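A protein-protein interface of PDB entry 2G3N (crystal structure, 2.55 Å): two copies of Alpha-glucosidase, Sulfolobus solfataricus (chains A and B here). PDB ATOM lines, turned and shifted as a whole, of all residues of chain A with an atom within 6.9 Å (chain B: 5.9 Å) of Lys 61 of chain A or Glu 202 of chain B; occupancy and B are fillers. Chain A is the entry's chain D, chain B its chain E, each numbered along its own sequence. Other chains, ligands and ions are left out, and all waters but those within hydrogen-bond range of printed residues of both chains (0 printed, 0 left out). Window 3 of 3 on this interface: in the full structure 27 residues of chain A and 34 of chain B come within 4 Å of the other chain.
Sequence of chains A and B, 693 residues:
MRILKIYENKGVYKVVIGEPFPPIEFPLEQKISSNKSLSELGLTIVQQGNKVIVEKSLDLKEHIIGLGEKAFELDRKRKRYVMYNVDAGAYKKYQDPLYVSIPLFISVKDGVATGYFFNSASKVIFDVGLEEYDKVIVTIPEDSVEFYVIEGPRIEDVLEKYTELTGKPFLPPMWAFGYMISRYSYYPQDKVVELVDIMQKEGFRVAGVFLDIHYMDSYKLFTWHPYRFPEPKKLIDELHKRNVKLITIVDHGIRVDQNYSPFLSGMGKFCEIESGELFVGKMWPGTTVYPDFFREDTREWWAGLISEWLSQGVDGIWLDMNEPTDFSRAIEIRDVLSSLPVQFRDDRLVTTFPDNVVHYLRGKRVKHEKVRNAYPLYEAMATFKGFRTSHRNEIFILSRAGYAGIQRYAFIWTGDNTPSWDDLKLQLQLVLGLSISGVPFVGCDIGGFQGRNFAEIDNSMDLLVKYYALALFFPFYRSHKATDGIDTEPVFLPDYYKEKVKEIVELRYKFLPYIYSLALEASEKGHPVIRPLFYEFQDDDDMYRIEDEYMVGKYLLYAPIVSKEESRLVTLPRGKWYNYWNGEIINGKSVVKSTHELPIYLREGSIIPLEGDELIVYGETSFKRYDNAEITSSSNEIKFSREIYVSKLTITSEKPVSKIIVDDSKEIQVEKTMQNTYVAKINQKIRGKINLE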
ATOM      1  N   LEU A  58      17.365 -19.679 -19.242  1.00  0.00           N
ATOM      2  CA  LEU A  58      16.795 -19.782 -17.910  1.00  0.00           C
ATOM      3  C   LEU A  58      17.717 -19.050 -16.945  1.00  0.00           C
ATOM      4  O   LEU A  58      18.871 -19.446 -16.762  1.00  0.00           O
ATOM      5  CB  LEU A  58      16.691 -21.254 -17.508  1.00  0.00           C
ATOM      6  CG  LEU A  58      16.053 -21.568 -16.157  1.00  0.00           C
ATOM      7  CD1 LEU A  58      14.549 -21.289 -16.209  1.00  0.00           C
ATOM      8  CD2 LEU A  58      16.310 -23.021 -15.812  1.00  0.00           C
ATOM      9  N   ASP A  59      17.216 -17.981 -16.336  1.00  0.00           N
ATOM     10  CA  ASP A  59      18.011 -17.212 -15.393  1.00  0.00           C
ATOM     11  C   ASP A  59      17.946 -17.805 -13.989  1.00  0.00           C
ATOM     12  O   ASP A  59      17.013 -18.543 -13.664  1.00  0.00           O
ATOM     13  CB  ASP A  59      17.533 -15.762 -15.362  1.00  0.00           C
ATOM     14  CG  ASP A  59      17.622 -15.092 -16.718  1.00  0.00           C
ATOM     15  OD1 ASP A  59      18.656 -15.262 -17.405  1.00  0.00           O
ATOM     16  OD2 ASP A  59      16.661 -14.384 -17.098  1.00  0.00           O
ATOM     17  N   LEU A  60      18.934 -17.473 -13.162  1.00  0.00           N
ATOM     18  CA  LEU A  60      18.989 -17.977 -11.795  1.00  0.00           C
ATOM     19  C   LEU A  60      17.713 -17.723 -10.996  1.00  0.00           C
ATOM     20  O   LEU A  60      17.226 -18.613 -10.296  1.00  0.00           O
ATOM     21  CB  LEU A  60      20.172 -17.359 -11.045  1.00  0.00           C
ATOM     22  CG  LEU A  60      21.566 -17.862 -11.393  1.00  0.00           C
ATOM     23  CD1 LEU A  60      22.592 -17.109 -10.567  1.00  0.00           C
ATOM     24  CD2 LEU A  60      21.648 -19.354 -11.123  1.00  0.00           C
ATOM     25  N   LYS A  61      17.177 -16.510 -11.104  1.00  0.00           N
ATOM     26  CA  LYS A  61      15.976 -16.130 -10.367  1.00  0.00           C
ATOM     27  C   LYS A  61      14.675 -16.431 -11.094  1.00  0.00           C
ATOM     28  O   LYS A  61      13.597 -16.169 -10.574  1.00  0.00           O
ATOM     29  CB  LYS A  61      16.020 -14.637 -10.027  1.00  0.00           C
ATOM     30  CG  LYS A  61      17.150 -14.213  -9.086  1.00  0.00           C
ATOM     31  CD  LYS A  61      16.879 -14.630  -7.645  1.00  0.00           C
ATOM     32  CE  LYS A  61      17.806 -13.881  -6.677  1.00  0.00           C
ATOM     33  NZ  LYS A  61      17.520 -14.175  -5.232  1.00  0.00           N
ATOM     34  N   GLU A  62      14.769 -16.978 -12.295  1.00  0.00           N
ATOM     35  CA  GLU A  62      13.580 -17.297 -13.071  1.00  0.00           C
ATOM     36  C   GLU A  62      12.816 -18.504 -12.506  1.00  0.00           C
ATOM     37  O   GLU A  62      13.425 -19.490 -12.102  1.00  0.00           O
ATOM     38  CB  GLU A  62      13.991 -17.560 -14.521  1.00  0.00           C
ATOM     39  CG  GLU A  62      12.846 -17.804 -15.485  1.00  0.00           C
ATOM     40  CD  GLU A  62      13.317 -17.806 -16.932  1.00  0.00           C
ATOM     41  OE1 GLU A  62      14.521 -17.541 -17.184  1.00  0.00           O
ATOM     42  OE2 GLU A  62      12.484 -18.063 -17.822  1.00  0.00           O
ATOM     43  N   HIS A  63      11.485 -18.419 -12.482  1.00  0.00           N
ATOM     44  CA  HIS A  63      10.649 -19.511 -11.981  1.00  0.00           C
ATOM     45  C   HIS A  63       9.930 -20.201 -13.132  1.00  0.00           C
ATOM     46  O   HIS A  63       9.497 -19.555 -14.084  1.00  0.00           O
ATOM     47  CB  HIS A  63       9.594 -18.984 -11.011  1.00  0.00           C
ATOM     48  CG  HIS A  63      10.155 -18.165  -9.896  1.00  0.00           C
ATOM     49  ND1 HIS A  63      10.984 -18.694  -8.929  1.00  0.00           N
ATOM     50  CD2 HIS A  63      10.036 -16.846  -9.613  1.00  0.00           C
ATOM     51  CE1 HIS A  63      11.353 -17.733  -8.099  1.00  0.00           C
ATOM     52  NE2 HIS A  63      10.792 -16.603  -8.492  1.00  0.00           N
ATOM     53  N   ASP A  75       7.944 -25.266  -8.266  1.00  0.00           N
ATOM     54  CA  ASP A  75       8.930 -24.603  -9.127  1.00  0.00           C
ATOM     55  C   ASP A  75       9.661 -25.798  -9.745  1.00  0.00           C
ATOM     56  O   ASP A  75      10.390 -26.510  -9.053  1.00  0.00           O
ATOM     57  CB  ASP A  75       9.915 -23.750  -8.321  1.00  0.00           C
ATOM     58  CG  ASP A  75      10.748 -22.803  -9.218  1.00  0.00           C
ATOM     59  OD1 ASP A  75      11.192 -23.222 -10.316  1.00  0.00           O
ATOM     60  OD2 ASP A  75      10.969 -21.634  -8.818  1.00  0.00           O
ATOM     61  N   LYS A  77      12.286 -26.238 -11.833  1.00  0.00           N
ATOM     62  CA  LYS A  77      13.695 -26.281 -12.231  1.00  0.00           C
ATOM     63  C   LYS A  77      14.498 -27.499 -11.744  1.00  0.00           C
ATOM     64  O   LYS A  77      14.193 -28.094 -10.720  1.00  0.00           O
ATOM     65  CB  LYS A  77      14.397 -24.996 -11.789  1.00  0.00           C
ATOM     66  CG  LYS A  77      13.830 -23.751 -12.444  1.00  0.00           C
ATOM     67  CD  LYS A  77      14.241 -22.475 -11.715  1.00  0.00           C
ATOM     68  CE  LYS A  77      15.710 -22.163 -11.887  1.00  0.00           C
ATOM     69  NZ  LYS A  77      16.054 -20.903 -11.162  1.00  0.00           N
ATOM     70  N   VAL A 108       8.210 -17.067 -15.043  1.00  0.00           N
ATOM     71  CA  VAL A 108       8.029 -15.807 -14.340  1.00  0.00           C
ATOM     72  C   VAL A 108       9.424 -15.259 -14.128  1.00  0.00           C
ATOM     73  O   VAL A 108      10.201 -15.777 -13.323  1.00  0.00           O
ATOM     74  CB  VAL A 108       7.338 -15.987 -12.981  1.00  0.00           C
ATOM     75  CG1 VAL A 108       7.064 -14.632 -12.374  1.00  0.00           C
ATOM     76  CG2 VAL A 108       6.039 -16.755 -13.157  1.00  0.00           C
ATOM     77  N   LYS A 109       9.741 -14.220 -14.887  1.00  0.00           N
ATOM     78  CA  LYS A 109      11.046 -13.588 -14.831  1.00  0.00           C
ATOM     79  C   LYS A 109      10.849 -12.103 -14.547  1.00  0.00           C
ATOM     80  O   LYS A 109      10.051 -11.432 -15.208  1.00  0.00           O
ATOM     81  CB  LYS A 109      11.763 -13.808 -16.164  1.00  0.00           C
ATOM     82  CG  LYS A 109      13.200 -13.349 -16.187  1.00  0.00           C
ATOM     83  CD  LYS A 109      13.924 -13.841 -17.426  1.00  0.00           C
ATOM     84  CE  LYS A 109      13.264 -13.366 -18.706  1.00  0.00           C
ATOM     85  NZ  LYS A 109      14.115 -13.690 -19.887  1.00  0.00           N
ATOM     86  N   ASP A 110      11.570 -11.596 -13.553  1.00  0.00           N
ATOM     87  CA  ASP A 110      11.453 -10.196 -13.171  1.00  0.00           C
ATOM     88  C   ASP A 110       9.985  -9.874 -12.860  1.00  0.00           C
ATOM     89  O   ASP A 110       9.497  -8.778 -13.156  1.00  0.00           O
ATOM     90  CB  ASP A 110      11.962  -9.280 -14.297  1.00  0.00           C
ATOM     91  CG  ASP A 110      13.435  -9.512 -14.629  1.00  0.00           C
ATOM     92  OD1 ASP A 110      14.269  -9.492 -13.698  1.00  0.00           O
ATOM     93  OD2 ASP A 110      13.766  -9.706 -15.823  1.00  0.00           O
ATOM     94  N   ASP A 541       9.541 -13.815  -4.681  1.00  0.00           N
ATOM     95  CA  ASP A 541      10.245 -15.091  -4.834  1.00  0.00           C
ATOM     96  C   ASP A 541       9.991 -16.113  -3.719  1.00  0.00           C
ATOM     97  O   ASP A 541       9.937 -17.312  -3.975  1.00  0.00           O
ATOM     98  CB  ASP A 541      11.749 -14.848  -4.990  1.00  0.00           C
ATOM     99  CG  ASP A 541      12.089 -14.078  -6.267  1.00  0.00           C
ATOM    100  OD1 ASP A 541      11.291 -14.130  -7.230  1.00  0.00           O
ATOM    101  OD2 ASP A 541      13.157 -13.428  -6.326  1.00  0.00           O
ATOM    102  N   ASP B 197      27.831 -13.671  -7.095  1.00  0.00           N
ATOM    103  CA  ASP B 197      27.437 -12.292  -6.857  1.00  0.00           C
ATOM    104  C   ASP B 197      26.185 -12.190  -6.005  1.00  0.00           C
ATOM    105  O   ASP B 197      26.130 -11.386  -5.076  1.00  0.00           O
ATOM    106  CB  ASP B 197      27.208 -11.549  -8.172  1.00  0.00           C
ATOM    107  CG  ASP B 197      28.495 -11.004  -8.767  1.00  0.00           C
ATOM    108  OD1 ASP B 197      29.435 -10.710  -7.992  1.00  0.00           O
ATOM    109  OD2 ASP B 197      28.569 -10.851 -10.004  1.00  0.00           O
ATOM    110  N   ILE B 198      25.174 -12.995  -6.315  1.00  0.00           N
ATOM    111  CA  ILE B 198      23.938 -12.960  -5.543  1.00  0.00           C
ATOM    112  C   ILE B 198      24.216 -13.385  -4.106  1.00  0.00           C
ATOM    113  O   ILE B 198      23.717 -12.775  -3.165  1.00  0.00           O
ATOM    114  CB  ILE B 198      22.867 -13.885  -6.153  1.00  0.00           C
ATOM    115  CG1 ILE B 198      22.598 -13.473  -7.598  1.00  0.00           C
ATOM    116  CG2 ILE B 198      21.568 -13.782  -5.358  1.00  0.00           C
ATOM    117  CD1 ILE B 198      21.595 -14.353  -8.312  1.00  0.00           C
ATOM    118  N   MET B 199      25.014 -14.434  -3.938  1.00  0.00           N
ATOM    119  CA  MET B 199      25.357 -14.912  -2.604  1.00  0.00           C
ATOM    120  C   MET B 199      26.002 -13.799  -1.778  1.00  0.00           C
ATOM    121  O   MET B 199      25.603 -13.540  -0.642  1.00  0.00           O
ATOM    122  CB  MET B 199      26.325 -16.097  -2.690  1.00  0.00           C
ATOM    123  CG  MET B 199      25.703 -17.422  -3.098  1.00  0.00           C
ATOM    124  SD  MET B 199      24.631 -18.114  -1.827  1.00  0.00           S
ATOM    125  CE  MET B 199      25.842 -18.964  -0.756  1.00  0.00           C
ATOM    126  N   GLN B 200      27.000 -13.138  -2.356  1.00  0.00           N
ATOM    127  CA  GLN B 200      27.700 -12.068  -1.651  1.00  0.00           C
ATOM    128  C   GLN B 200      26.810 -10.860  -1.402  1.00  0.00           C
ATOM    129  O   GLN B 200      26.844 -10.258  -0.326  1.00  0.00           O
ATOM    130  CB  GLN B 200      28.951 -11.652  -2.431  1.00  0.00           C
ATOM    131  CG  GLN B 200      29.944 -12.794  -2.620  1.00  0.00           C
ATOM    132  CD  GLN B 200      31.247 -12.348  -3.242  1.00  0.00           C
ATOM    133  OE1 GLN B 200      31.252 -11.634  -4.244  1.00  0.00           O
ATOM    134  NE2 GLN B 200      32.365 -12.780  -2.658  1.00  0.00           N
ATOM    135  N   LYS B 201      26.002 -10.512  -2.392  1.00  0.00           N
ATOM    136  CA  LYS B 201      25.112  -9.376  -2.253  1.00  0.00           C
ATOM    137  C   LYS B 201      24.119  -9.592  -1.112  1.00  0.00           C
ATOM    138  O   LYS B 201      23.753  -8.645  -0.412  1.00  0.00           O
ATOM    139  CB  LYS B 201      24.364  -9.133  -3.561  1.00  0.00           C
ATOM    140  CG  LYS B 201      23.372  -7.993  -3.496  1.00  0.00           C
ATOM    141  CD  LYS B 201      22.676  -7.793  -4.830  1.00  0.00           C
ATOM    142  CE  LYS B 201      21.660  -6.659  -4.760  1.00  0.00           C
ATOM    143  NZ  LYS B 201      20.587  -6.946  -3.765  1.00  0.00           N
ATOM    144  N   GLU B 202      23.683 -10.834  -0.914  1.00  0.00           N
ATOM    145  CA  GLU B 202      22.734 -11.112   0.157  1.00  0.00           C
ATOM    146  C   GLU B 202      23.390 -11.406   1.507  1.00  0.00           C
ATOM    147  O   GLU B 202      22.736 -11.868   2.442  1.00  0.00           O
ATOM    148  CB  GLU B 202      21.782 -12.238  -0.256  1.00  0.00           C
ATOM    149  CG  GLU B 202      20.725 -11.757  -1.262  1.00  0.00           C
ATOM    150  CD  GLU B 202      19.589 -12.753  -1.478  1.00  0.00           C
ATOM    151  OE1 GLU B 202      19.150 -13.380  -0.486  1.00  0.00           O
ATOM    152  OE2 GLU B 202      19.120 -12.895  -2.635  1.00  0.00           O
ATOM    153  N   GLY B 203      24.688 -11.133   1.602  1.00  0.00           N
ATOM    154  CA  GLY B 203      25.384 -11.318   2.856  1.00  0.00           C
ATOM    155  C   GLY B 203      26.086 -12.623   3.164  1.00  0.00           C
ATOM    156  O   GLY B 203      26.549 -12.803   4.287  1.00  0.00           O
ATOM    157  N   PHE B 204      26.180 -13.535   2.208  1.00  0.00           N
ATOM    158  CA  PHE B 204      26.858 -14.786   2.490  1.00  0.00           C
ATOM    159  C   PHE B 204      28.308 -14.699   2.086  1.00  0.00           C
ATOM    160  O   PHE B 204      28.635 -14.388   0.948  1.00  0.00           O
ATOM    161  CB  PHE B 204      26.177 -15.959   1.776  1.00  0.00           C
ATOM    162  CG  PHE B 204      24.791 -16.236   2.272  1.00  0.00           C
ATOM    163  CD1 PHE B 204      23.694 -15.575   1.720  1.00  0.00           C
ATOM    164  CD2 PHE B 204      24.585 -17.114   3.327  1.00  0.00           C
ATOM    165  CE1 PHE B 204      22.420 -15.787   2.211  1.00  0.00           C
ATOM    166  CE2 PHE B 204      23.316 -17.332   3.829  1.00  0.00           C
ATOM    167  CZ  PHE B 204      22.227 -16.667   3.271  1.00  0.00           C
ATOM    168  N   PRO B 490      21.383 -20.801  -0.219  1.00  0.00           N
ATOM    169  CA  PRO B 490      20.611 -19.971   0.711  1.00  0.00           C
ATOM    170  C   PRO B 490      19.831 -18.824   0.060  1.00  0.00           C
ATOM    171  O   PRO B 490      18.726 -18.489   0.500  1.00  0.00           O
ATOM    172  CB  PRO B 490      21.674 -19.465   1.681  1.00  0.00           C
ATOM    173  CG  PRO B 490      22.679 -20.556   1.673  1.00  0.00           C
ATOM    174  CD  PRO B 490      22.785 -20.890   0.213  1.00  0.00           C
ATOM    175  N   VAL B 491      20.403 -18.227  -0.980  1.00  0.00           N
ATOM    176  CA  VAL B 491      19.747 -17.127  -1.666  1.00  0.00           C
ATOM    177  C   VAL B 491      18.414 -17.507  -2.306  1.00  0.00           C
ATOM    178  O   VAL B 491      17.637 -16.629  -2.685  1.00  0.00           O
ATOM    179  CB  VAL B 491      20.655 -16.523  -2.759  1.00  0.00           C
ATOM    180  CG1 VAL B 491      21.868 -15.870  -2.121  1.00  0.00           C
ATOM    181  CG2 VAL B 491      21.077 -17.601  -3.747  1.00  0.00           C
ATOM    182  N   PHE B 492      18.146 -18.806  -2.430  1.00  0.00           N
ATOM    183  CA  PHE B 492      16.896 -19.262  -3.031  1.00  0.00           C
ATOM    184  C   PHE B 492      15.857 -19.670  -1.999  1.00  0.00           C
ATOM    185  O   PHE B 492      14.791 -20.172  -2.356  1.00  0.00           O
ATOM    186  CB  PHE B 492      17.142 -20.443  -3.973  1.00  0.00           C
ATOM    187  CG  PHE B 492      18.038 -20.118  -5.129  1.00  0.00           C
ATOM    188  CD1 PHE B 492      17.684 -19.127  -6.039  1.00  0.00           C
ATOM    189  CD2 PHE B 492      19.242 -20.796  -5.305  1.00  0.00           C
ATOM    190  CE1 PHE B 492      18.513 -18.810  -7.109  1.00  0.00           C
ATOM    191  CE2 PHE B 492      20.083 -20.491  -6.371  1.00  0.00           C
ATOM    192  CZ  PHE B 492      19.719 -19.492  -7.279  1.00  0.00           C
ATOM    193  N   LYS B 498      16.244 -18.386   4.970  1.00  0.00           N
ATOM    194  CA  LYS B 498      17.467 -17.750   4.511  1.00  0.00           C
ATOM    195  C   LYS B 498      18.174 -17.052   5.672  1.00  0.00           C
ATOM    196  O   LYS B 498      19.398 -17.133   5.798  1.00  0.00           O
ATOM    197  CB  LYS B 498      17.156 -16.740   3.404  1.00  0.00           C
ATOM    198  CG  LYS B 498      18.357 -15.918   2.971  1.00  0.00           C
ATOM    199  CD  LYS B 498      18.126 -15.246   1.630  1.00  0.00           C
ATOM    200  CE  LYS B 498      16.918 -14.308   1.655  1.00  0.00           C
ATOM    201  NZ  LYS B 498      16.605 -13.756   0.297  1.00  0.00           N
ATOM    202  N   LYS B 502      21.913 -17.810   7.206  1.00  0.00           N
ATOM    203  CA  LYS B 502      22.811 -16.665   7.261  1.00  0.00           C
ATOM    204  C   LYS B 502      23.417 -16.517   8.664  1.00  0.00           C
ATOM    205  O   LYS B 502      24.620 -16.306   8.806  1.00  0.00           O
ATOM    206  CB  LYS B 502      22.031 -15.402   6.889  1.00  0.00           C
ATOM    207  CG  LYS B 502      22.853 -14.160   6.613  1.00  0.00           C
ATOM    208  CD  LYS B 502      21.929 -13.053   6.100  1.00  0.00           C
ATOM    209  CE  LYS B 502      22.681 -11.795   5.701  1.00  0.00           C
ATOM    210  NZ  LYS B 502      23.381 -11.167   6.857  1.00  0.00           N
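NZ of Lys 61 of chain A is in salt-bridge range of OE2 of Glu 202 of chain B (3.3 Å).
The side-chain amino group (NZ) of Lys 498 of chain B lies within salt-bridge range of the side-chain carboxylate (OE1) of Glu 202 of chain B, 2.7 Å away. NZ of Lys 77 of chain A lies within hydrogen-bond range of O of Leu 60 of chain A, at 2.7 Å.
Among the printed residues, pairs that only touch across the chains: Leu 60 of chain A with Phe 492 of chain B (3.4 Å), Lys 61 of chain A with Val 491 of chain B (3.5 Å), Leu 60 of chain A with Ile 198 of chain B (3.7 Å) and Lys 61 of chain A with Ile 198 of chain B (3.99 Å).
Of the printed residues of chain B, Lys 61 of chain A touches Ile 198 (3.99 Å), Glu 202 (3.3 Å) and Val 491 (3.5 Å). Of the printed residues of chain A, Glu 202 of chain B touches Lys 61. Of the printed residues of chain A, Ile 198 of chain B touches Leu 60 (3.7 Å) and Lys 61 (3.99 Å). Of the printed residues of chain A, Phe 492 of chain B touches Leu 60. Of the printed residues of chain B, Leu 60 of chain A touches Ile 198 (3.7 Å) and Phe 492 (3.4 Å). Of the printed residues of chain A, Val 491 of chain B touches Lys 61. Asp 75 of chain A touches none of the printed residues of chain B. The nearest printed residue of chain B that does not touch Lys 61 of chain A is Phe 492 of chain B (4.5 Å). The nearest printed residue of chain A that does not touch Glu 202 of chain B is Asp 541 of chain A (7.0 Å).
Printed residues of chain B that touch a printed residue of chain A: Ile 198, Glu 202, Val 491 and Phe 492. Hydrophobic or aromatic side chains of chain B within 4 Å of the printed part of chain A: Ile 198 and Phe 492. Among the printed residues, 5 pairs touch across the chains. Among the printed residues, Asp or Glu carboxylates within 4 Å of a Lys or Arg side-chain nitrogen of the other chain: Lys 61 of chain A with Glu 202 of chain B (3.3 Å).
No position is printed for both chains. Of the 5 pairs that touch across the chains among the printed residues, none has its exchanged pair printed and touching as well.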
